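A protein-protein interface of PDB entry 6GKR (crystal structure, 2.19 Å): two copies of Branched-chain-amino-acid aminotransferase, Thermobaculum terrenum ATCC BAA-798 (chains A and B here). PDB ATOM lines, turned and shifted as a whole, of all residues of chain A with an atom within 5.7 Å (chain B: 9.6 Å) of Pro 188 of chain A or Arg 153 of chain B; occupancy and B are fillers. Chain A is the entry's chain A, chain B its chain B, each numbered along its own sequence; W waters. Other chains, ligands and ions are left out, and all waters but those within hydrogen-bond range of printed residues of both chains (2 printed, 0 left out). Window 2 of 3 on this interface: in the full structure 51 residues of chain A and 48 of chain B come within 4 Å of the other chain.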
ATOM      1  N   SER A 146      -2.859 -10.061  17.200  1.00  0.00           N
ATOM      2  CA  SER A 146      -2.401 -10.897  16.097  1.00  0.00           C
ATOM      3  C   SER A 146      -2.410 -10.090  14.797  1.00  0.00           C
ATOM      4  O   SER A 146      -2.027 -10.617  13.758  1.00  0.00           O
ATOM      5  CB  SER A 146      -3.268 -12.104  15.934  1.00  0.00           C
ATOM      6  OG  SER A 146      -4.585 -11.710  15.548  1.00  0.00           O
ATOM      7  N   TRP A 147      -2.895  -8.836  14.828  1.00  0.00           N
ATOM      8  CA  TRP A 147      -2.817  -7.937  13.682  1.00  0.00           C
ATOM      9  C   TRP A 147      -1.583  -7.045  13.827  1.00  0.00           C
ATOM     10  O   TRP A 147      -1.221  -6.652  14.955  1.00  0.00           O
ATOM     11  CB  TRP A 147      -4.080  -7.083  13.603  1.00  0.00           C
ATOM     12  CG  TRP A 147      -5.303  -7.908  13.362  1.00  0.00           C
ATOM     13  CD1 TRP A 147      -6.165  -8.378  14.300  1.00  0.00           C
ATOM     14  CD2 TRP A 147      -5.750  -8.437  12.106  1.00  0.00           C
ATOM     15  NE1 TRP A 147      -7.119  -9.155  13.712  1.00  0.00           N
ATOM     16  CE2 TRP A 147      -6.917  -9.191  12.366  1.00  0.00           C
ATOM     17  CE3 TRP A 147      -5.306  -8.319  10.779  1.00  0.00           C
ATOM     18  CZ2 TRP A 147      -7.641  -9.838  11.355  1.00  0.00           C
ATOM     19  CZ3 TRP A 147      -6.030  -8.943   9.775  1.00  0.00           C
ATOM     20  CH2 TRP A 147      -7.160  -9.716  10.061  1.00  0.00           C
ATOM     21  N   THR A 148      -0.935  -6.732  12.694  1.00  0.00           N
ATOM     22  CA  THR A 148       0.338  -6.021  12.703  1.00  0.00           C
ATOM     23  C   THR A 148       0.092  -4.528  12.546  1.00  0.00           C
ATOM     24  O   THR A 148      -0.770  -4.133  11.765  1.00  0.00           O
ATOM     25  CB  THR A 148       1.233  -6.551  11.571  1.00  0.00           C
ATOM     26  OG1 THR A 148       1.242  -7.972  11.746  1.00  0.00           O
ATOM     27  CG2 THR A 148       2.647  -6.022  11.605  1.00  0.00           C
ATOM     28  N   ARG A 149       0.901  -3.705  13.225  1.00  0.00           N
ATOM     29  CA  ARG A 149       0.779  -2.255  13.105  1.00  0.00           C
ATOM     30  C   ARG A 149       1.168  -1.801  11.699  1.00  0.00           C
ATOM     31  O   ARG A 149       2.187  -2.257  11.160  1.00  0.00           O
ATOM     32  CB  ARG A 149       1.663  -1.563  14.148  1.00  0.00           C
ATOM     33  CG  ARG A 149       1.405  -0.075  14.280  1.00  0.00           C
ATOM     34  CD  ARG A 149      -0.050   0.249  14.568  1.00  0.00           C
ATOM     35  NE  ARG A 149      -0.310   1.666  14.742  1.00  0.00           N
ATOM     36  CZ  ARG A 149      -1.474   2.262  14.543  1.00  0.00           C
ATOM     37  NH1 ARG A 149      -2.508   1.594  14.047  1.00  0.00           N
ATOM     38  NH2 ARG A 149      -1.588   3.545  14.825  1.00  0.00           N
ATOM     39  N   ILE A 150       0.407  -0.849  11.143  1.00  0.00           N
ATOM     40  CA  ILE A 150       0.817  -0.127   9.937  1.00  0.00           C
ATOM     41  C   ILE A 150       2.235   0.423  10.101  1.00  0.00           C
ATOM     42  O   ILE A 150       2.649   0.771  11.216  1.00  0.00           O
ATOM     43  CB  ILE A 150      -0.200   0.995   9.606  1.00  0.00           C
ATOM     44  CG1 ILE A 150      -0.540   1.816  10.852  1.00  0.00           C
ATOM     45  CG2 ILE A 150      -1.469   0.441   8.939  1.00  0.00           C
ATOM     46  CD1 ILE A 150      -1.158   3.174  10.585  1.00  0.00           C
ATOM     47  N   ASN A 151       2.961   0.569   8.972  1.00  0.00           N
ATOM     48  CA  ASN A 151       4.337   1.056   8.998  1.00  0.00           C
ATOM     49  C   ASN A 151       4.541   2.078   7.874  1.00  0.00           C
ATOM     50  O   ASN A 151       3.633   2.292   7.056  1.00  0.00           O
ATOM     51  CB  ASN A 151       5.354  -0.094   8.939  1.00  0.00           C
ATOM     52  CG  ASN A 151       5.385  -0.851   7.614  1.00  0.00           C
ATOM     53  OD1 ASN A 151       4.511  -0.700   6.775  1.00  0.00           O
ATOM     54  ND2 ASN A 151       6.394  -1.690   7.410  1.00  0.00           N
ATOM     55  N   ASN A 167      -6.794   0.065  11.171  1.00  0.00           N
ATOM     56  CA  ASN A 167      -5.805  -0.857  11.699  1.00  0.00           C
ATOM     57  C   ASN A 167      -5.961  -0.970  13.222  1.00  0.00           C
ATOM     58  O   ASN A 167      -5.999  -2.086  13.762  1.00  0.00           O
ATOM     59  CB  ASN A 167      -4.398  -0.514  11.178  1.00  0.00           C
ATOM     60  CG  ASN A 167      -3.279  -1.321  11.800  1.00  0.00           C
ATOM     61  OD1 ASN A 167      -2.514  -0.808  12.622  1.00  0.00           O
ATOM     62  ND2 ASN A 167      -3.128  -2.555  11.366  1.00  0.00           N
ATOM     63  N   LEU A 186       2.540  -5.191  17.715  1.00  0.00           N
ATOM     64  CA  LEU A 186       3.865  -5.420  17.158  1.00  0.00           C
ATOM     65  C   LEU A 186       3.944  -4.818  15.754  1.00  0.00           C
ATOM     66  O   LEU A 186       2.954  -4.833  15.015  1.00  0.00           O
ATOM     67  CB  LEU A 186       4.136  -6.921  17.108  1.00  0.00           C
ATOM     68  CG  LEU A 186       3.889  -7.677  18.413  1.00  0.00           C
ATOM     69  CD1 LEU A 186       4.012  -9.180  18.164  1.00  0.00           C
ATOM     70  CD2 LEU A 186       4.839  -7.197  19.504  1.00  0.00           C
ATOM     71  N   ASN A 187       5.137  -4.324  15.379  1.00  0.00           N
ATOM     72  CA  ASN A 187       5.358  -3.818  14.026  1.00  0.00           C
ATOM     73  C   ASN A 187       5.672  -5.022  13.116  1.00  0.00           C
ATOM     74  O   ASN A 187       5.747  -6.162  13.609  1.00  0.00           O
ATOM     75  CB  ASN A 187       6.406  -2.688  14.011  1.00  0.00           C
ATOM     76  CG  ASN A 187       7.814  -3.133  14.396  1.00  0.00           C
ATOM     77  OD1 ASN A 187       8.150  -4.317  14.346  1.00  0.00           O
ATOM     78  ND2 ASN A 187       8.658  -2.205  14.810  1.00  0.00           N
ATOM     79  N   PRO A 188       5.815  -4.826  11.777  1.00  0.00           N
ATOM     80  CA  PRO A 188       6.093  -5.932  10.857  1.00  0.00           C
ATOM     81  C   PRO A 188       7.342  -6.753  11.175  1.00  0.00           C
ATOM     82  O   PRO A 188       7.364  -7.933  10.886  1.00  0.00           O
ATOM     83  CB  PRO A 188       6.175  -5.247   9.483  1.00  0.00           C
ATOM     84  CG  PRO A 188       5.252  -4.049   9.644  1.00  0.00           C
ATOM     85  CD  PRO A 188       5.559  -3.570  11.047  1.00  0.00           C
ATOM     86  N   GLU A 189       8.307  -6.156  11.881  1.00  0.00           N
ATOM     87  CA  GLU A 189       9.536  -6.836  12.253  1.00  0.00           C
ATOM     88  C   GLU A 189       9.353  -7.617  13.567  1.00  0.00           C
ATOM     89  O   GLU A 189      10.291  -8.263  14.042  1.00  0.00           O
ATOM     90  CB  GLU A 189      10.708  -5.846  12.350  1.00  0.00           C
ATOM     91  CG  GLU A 189      11.261  -5.468  10.986  1.00  0.00           C
ATOM     92  CD  GLU A 189      10.313  -4.574  10.189  1.00  0.00           C
ATOM     93  OE1 GLU A 189       9.792  -3.610  10.793  1.00  0.00           O
ATOM     94  OE2 GLU A 189      10.045  -4.857   8.972  1.00  0.00           O
ATOM     95  N   GLY A 190       8.182  -7.495  14.190  1.00  0.00           N
ATOM     96  CA  GLY A 190       7.870  -8.233  15.394  1.00  0.00           C
ATOM     97  C   GLY A 190       8.256  -7.458  16.657  1.00  0.00           C
ATOM     98  O   GLY A 190       8.268  -8.055  17.739  1.00  0.00           O
ATOM     99  N   LYS A 191       8.559  -6.149  16.532  1.00  0.00           N
ATOM    100  CA  LYS A 191       8.956  -5.385  17.716  1.00  0.00           C
ATOM    101  C   LYS A 191       7.757  -4.591  18.244  1.00  0.00           C
ATOM    102  O   LYS A 191       6.798  -4.349  17.510  1.00  0.00           O
ATOM    103  CB  LYS A 191      10.155  -4.463  17.424  1.00  0.00           C
ATOM    104  CG  LYS A 191      11.380  -5.105  16.760  1.00  0.00           C
ATOM    105  CD  LYS A 191      11.886  -6.289  17.612  1.00  0.00           C
ATOM    106  CE  LYS A 191      13.210  -6.895  17.176  1.00  0.00           C
ATOM    107  NZ  LYS A 191      13.466  -8.186  17.870  1.00  0.00           N
ATOM    108  N   ARG B 149       1.714  -1.665  -1.244  1.00  0.00           N
ATOM    109  CA  ARG B 149       0.312  -1.976  -1.018  1.00  0.00           C
ATOM    110  C   ARG B 149       0.123  -2.563   0.389  1.00  0.00           C
ATOM    111  O   ARG B 149       0.917  -3.397   0.834  1.00  0.00           O
ATOM    112  CB  ARG B 149      -0.177  -2.965  -2.077  1.00  0.00           C
ATOM    113  CG  ARG B 149      -1.681  -3.257  -2.028  1.00  0.00           C
ATOM    114  CD  ARG B 149      -2.399  -1.942  -2.321  1.00  0.00           C
ATOM    115  NE  ARG B 149      -3.838  -2.103  -2.437  1.00  0.00           N
ATOM    116  CZ  ARG B 149      -4.756  -1.219  -2.109  1.00  0.00           C
ATOM    117  NH1 ARG B 149      -4.393  -0.057  -1.591  1.00  0.00           N
ATOM    118  NH2 ARG B 149      -6.027  -1.555  -2.243  1.00  0.00           N
ATOM    119  N   ILE B 150      -0.965  -2.173   1.070  1.00  0.00           N
ATOM    120  CA  ILE B 150      -1.444  -2.842   2.272  1.00  0.00           C
ATOM    121  C   ILE B 150      -1.522  -4.356   2.030  1.00  0.00           C
ATOM    122  O   ILE B 150      -1.739  -4.831   0.918  1.00  0.00           O
ATOM    123  CB  ILE B 150      -2.834  -2.268   2.666  1.00  0.00           C
ATOM    124  CG1 ILE B 150      -3.781  -2.180   1.460  1.00  0.00           C
ATOM    125  CG2 ILE B 150      -2.750  -0.913   3.361  1.00  0.00           C
ATOM    126  CD1 ILE B 150      -5.253  -2.080   1.800  1.00  0.00           C
ATOM    127  N   ASN B 151      -1.367  -5.142   3.104  1.00  0.00           N
ATOM    128  CA  ASN B 151      -1.415  -6.605   3.045  1.00  0.00           C
ATOM    129  C   ASN B 151      -2.243  -7.129   4.221  1.00  0.00           C
ATOM    130  O   ASN B 151      -2.681  -6.350   5.072  1.00  0.00           O
ATOM    131  CB  ASN B 151      -0.004  -7.221   3.012  1.00  0.00           C
ATOM    132  CG  ASN B 151       0.804  -7.028   4.292  1.00  0.00           C
ATOM    133  OD1 ASN B 151       0.437  -6.261   5.174  1.00  0.00           O
ATOM    134  ND2 ASN B 151       1.929  -7.722   4.413  1.00  0.00           N
ATOM    135  N   GLU B 152      -2.444  -8.453   4.269  1.00  0.00           N
ATOM    136  CA  GLU B 152      -3.269  -9.069   5.301  1.00  0.00           C
ATOM    137  C   GLU B 152      -2.713  -8.859   6.706  1.00  0.00           C
ATOM    138  O   GLU B 152      -3.461  -8.965   7.672  1.00  0.00           O
ATOM    139  CB  GLU B 152      -3.477 -10.544   5.018  1.00  0.00           C
ATOM    140  CG  GLU B 152      -4.420 -10.707   3.835  1.00  0.00           C
ATOM    141  CD  GLU B 152      -5.773 -11.228   4.238  1.00  0.00           C
ATOM    142  OE1 GLU B 152      -5.833 -11.946   5.259  1.00  0.00           O
ATOM    143  OE2 GLU B 152      -6.734 -10.981   3.509  1.00  0.00           O
ATOM    144  N   ARG B 153      -1.407  -8.591   6.832  1.00  0.00           N
ATOM    145  CA  ARG B 153      -0.838  -8.331   8.148  1.00  0.00           C
ATOM    146  C   ARG B 153      -1.464  -7.088   8.786  1.00  0.00           C
ATOM    147  O   ARG B 153      -1.667  -7.101  10.000  1.00  0.00           O
ATOM    148  CB  ARG B 153       0.693  -8.296   8.154  1.00  0.00           C
ATOM    149  CG  ARG B 153       1.352  -9.554   7.591  1.00  0.00           C
ATOM    150  CD  ARG B 153       2.277 -10.160   8.656  1.00  0.00           C
ATOM    151  NE  ARG B 153       3.502  -9.413   8.700  1.00  0.00           N
ATOM    152  CZ  ARG B 153       4.374  -9.260   9.693  1.00  0.00           C
ATOM    153  NH1 ARG B 153       4.046  -9.368  10.966  1.00  0.00           N
ATOM    154  NH2 ARG B 153       5.603  -8.907   9.379  1.00  0.00           N
ATOM    155  N   VAL B 154      -1.769  -6.038   7.978  1.00  0.00           N
ATOM    156  CA  VAL B 154      -2.040  -4.715   8.516  1.00  0.00           C
ATOM    157  C   VAL B 154      -3.447  -4.219   8.185  1.00  0.00           C
ATOM    158  O   VAL B 154      -4.052  -3.553   9.023  1.00  0.00           O
ATOM    159  CB  VAL B 154      -0.962  -3.667   8.163  1.00  0.00           C
ATOM    160  CG1 VAL B 154       0.411  -4.089   8.629  1.00  0.00           C
ATOM    161  CG2 VAL B 154      -0.941  -3.270   6.692  1.00  0.00           C
ATOM    162  N   LEU B 155      -3.953  -4.523   6.990  1.00  0.00           N
ATOM    163  CA  LEU B 155      -5.205  -4.006   6.448  1.00  0.00           C
ATOM    164  C   LEU B 155      -5.601  -4.895   5.260  1.00  0.00           C
ATOM    165  O   LEU B 155      -5.209  -4.636   4.122  1.00  0.00           O
ATOM    166  CB  LEU B 155      -5.010  -2.581   5.923  1.00  0.00           C
ATOM    167  CG  LEU B 155      -5.289  -1.371   6.821  1.00  0.00           C
ATOM    168  CD1 LEU B 155      -5.650  -0.188   5.938  1.00  0.00           C
ATOM    169  CD2 LEU B 155      -6.423  -1.611   7.819  1.00  0.00           C
ATOM    170  N   PRO B 156      -6.332  -6.003   5.496  1.00  0.00           N
ATOM    171  CA  PRO B 156      -6.631  -6.950   4.435  1.00  0.00           C
ATOM    172  C   PRO B 156      -7.236  -6.285   3.198  1.00  0.00           C
ATOM    173  O   PRO B 156      -8.229  -5.574   3.269  1.00  0.00           O
ATOM    174  CB  PRO B 156      -7.586  -7.939   5.110  1.00  0.00           C
ATOM    175  CG  PRO B 156      -7.188  -7.865   6.577  1.00  0.00           C
ATOM    176  CD  PRO B 156      -6.911  -6.400   6.796  1.00  0.00           C
ATOM    177  N   PRO B 157      -6.547  -6.377   2.039  1.00  0.00           N
ATOM    178  CA  PRO B 157      -7.091  -5.837   0.791  1.00  0.00           C
ATOM    179  C   PRO B 157      -8.385  -6.454   0.272  1.00  0.00           C
ATOM    180  O   PRO B 157      -9.071  -5.802  -0.520  1.00  0.00           O
ATOM    181  CB  PRO B 157      -5.949  -5.937  -0.215  1.00  0.00           C
ATOM    182  CG  PRO B 157      -4.932  -6.864   0.421  1.00  0.00           C
ATOM    183  CD  PRO B 157      -5.151  -6.843   1.914  1.00  0.00           C
ATOM    184  N   ARG B 158      -8.723  -7.667   0.740  1.00  0.00           N
ATOM    185  CA  ARG B 158      -9.991  -8.342   0.448  1.00  0.00           C
ATOM    186  C   ARG B 158     -11.181  -7.470   0.879  1.00  0.00           C
ATOM    187  O   ARG B 158     -12.252  -7.507   0.259  1.00  0.00           O
ATOM    188  CB  ARG B 158     -10.010  -9.692   1.202  1.00  0.00           C
ATOM    189  CG  ARG B 158     -11.205 -10.615   1.020  1.00  0.00           C
ATOM    190  CD  ARG B 158     -10.902 -12.056   1.448  1.00  0.00           C
ATOM    191  NE  ARG B 158     -10.028 -12.811   0.510  1.00  0.00           N
ATOM    192  CZ  ARG B 158      -8.719 -13.036   0.700  1.00  0.00           C
ATOM    193  NH1 ARG B 158      -8.216 -12.834   1.894  1.00  0.00           N
ATOM    194  NH2 ARG B 158      -7.910 -13.400  -0.286  1.00  0.00           N
ATOM    195  N   PRO B 188       4.412  -6.041  -0.085  1.00  0.00           N
ATOM    196  CA  PRO B 188       5.601  -5.976   0.764  1.00  0.00           C
ATOM    197  C   PRO B 188       6.747  -6.900   0.342  1.00  0.00           C
ATOM    198  O   PRO B 188       7.896  -6.597   0.609  1.00  0.00           O
ATOM    199  CB  PRO B 188       5.067  -6.308   2.168  1.00  0.00           C
ATOM    200  CG  PRO B 188       3.649  -5.780   2.111  1.00  0.00           C
ATOM    201  CD  PRO B 188       3.181  -6.220   0.715  1.00  0.00           C
ATOM    202  N   GLU B 189       6.431  -7.982  -0.369  1.00  0.00           N
ATOM    203  CA  GLU B 189       7.436  -8.926  -0.846  1.00  0.00           C
ATOM    204  C   GLU B 189       8.032  -8.446  -2.171  1.00  0.00           C
ATOM    205  O   GLU B 189       9.002  -9.023  -2.639  1.00  0.00           O
ATOM    206  CB  GLU B 189       6.877 -10.350  -0.951  1.00  0.00           C
ATOM    207  CG  GLU B 189       6.724 -11.028   0.403  1.00  0.00           C
ATOM    208  CD  GLU B 189       5.638 -10.428   1.295  1.00  0.00           C
ATOM    209  OE1 GLU B 189       4.511 -10.207   0.781  1.00  0.00           O
ATOM    210  OE2 GLU B 189       5.929 -10.130   2.484  1.00  0.00           O
ATOM    211  N   GLY B 216      -2.394 -10.098  -2.545  1.00  0.00           N
ATOM    212  CA  GLY B 216      -2.789  -8.950  -1.747  1.00  0.00           C
ATOM    213  C   GLY B 216      -3.590  -7.934  -2.570  1.00  0.00           C
ATOM    214  O   GLY B 216      -3.168  -6.792  -2.729  1.00  0.00           O
HETATM  215  O   HOH W   1      -0.937 -10.025  11.497  1.00  0.00           O
HETATM  216  O   HOH W   2       4.641  -8.682  13.778  1.00  0.00           O
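The guanidinium group (NH2) of Arg 153 of chain B lies within hydrogen-bond range of the backbone carbonyl oxygen (O) of Pro 188 of chain A. The side-chain amide nitrogen (ND2) of Asn 167 of chain A sits at hydrogen-bond distance from the backbone carbonyl oxygen (O) of Val 154 of chain B, 2.7 Å away. The backbone NH (N) of Thr 148 of chain A sits at hydrogen-bond distance from the backbone carbonyl oxygen (O) of Arg 153 of chain B (2.8 Å).
The backbone NH (N) of Arg 153 of chain B lies close to the side-chain amide oxygen (OD1) of Asn 151 of chain B (3.4 Å). OE2 of Glu 152 of chain B is in salt-bridge range of NH1 of Arg 158 of chain B (2.9 Å). The guanidinium group of Arg 149 of chain A is in hydrogen-bond range of the side-chain amide oxygen of Asn 167 of chain A (2.8 Å). The backbone carbonyl oxygen (O) of Thr 148 of chain A is in hydrogen-bond range of the side-chain amide nitrogen (ND2) of Asn 167 of chain A (2.9 Å). N of Ile 150 of chain A lies within hydrogen-bond range of OD1 of Asn 167 of chain A. The backbone NH of Arg 149 of chain A is in hydrogen-bond range of the backbone carbonyl oxygen of Leu 186 of chain A (2.9 Å).
Among the printed residues, pairs that only touch across the chains: Trp 147 of chain A with Glu 152 of chain B (3.3 Å), Trp 147 of chain A with Arg 153 of chain B (3.8 Å), Trp 147 of chain A with Pro 156 of chain B (3.6 Å), Thr 148 of chain A with Val 154 of chain B (3.4 Å), Arg 149 of chain A with Val 154 of chain B (3.6 Å) and Asn 167 of chain A with Leu 155 of chain B (3.8 Å).
Of the printed residues of chain B, Arg 149 of chain A touches Val 154 (3.6 Å). Printed residues of chain B within 4 Å of Asn 167 of chain A: Val 154 (2.7 Å) and Leu 155 (3.8 Å). Pro 188 of chain A touches just one residue of chain B: Arg 153. Ile 150 of chain B touches none of the printed residues of chain A. Asn 151 of chain B touches none of the printed residues of chain A. Arg 153 of chain B touches just these residues of chain A: Trp 147 (3.8 Å), Thr 148 (2.8 Å) and Pro 188 (2.5 Å). Of the printed residues of chain A, Val 154 of chain B touches Thr 148 (3.4 Å), Arg 149 (3.6 Å) and Asn 167 (2.7 Å). Of the printed residues of chain A, Leu 155 of chain B touches Asn 167. Of the printed residues of chain A, Pro 156 of chain B touches Trp 147 (3.6 Å). The nearest printed residue of chain A that does not touch Pro 156 of chain B is Asn 167 of chain A (7.1 Å).
Of the 13 printed residues of chain A, 5 touch a printed residue of chain B. Hydrophobic or aromatic side chains of chain A that line the printed part of chain B: Trp 147 and Pro 188. Of the 13 printed residues of chain B, 5 touch a printed residue of chain A. Printed residues of chain B that touch a printed residue of chain A: Glu 152, Arg 153, Val 154, Leu 155 and Pro 156. Hydrophobic or aromatic side chains of chain B that line the printed part of chain A: Val 154, Leu 155 and Pro 156.
5 positions are printed for both chains.
Water W1 lies within hydrogen-bond range of O of Ser 146 of chain A, OG1 of Thr 148 of chain A and O of Arg 153 of chain B. Water W2 bridges the backbone carbonyl oxygen of Asn 187 of chain A (2.8 Å) and the guanidinium group of Arg 153 of chain B (3.0 Å).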
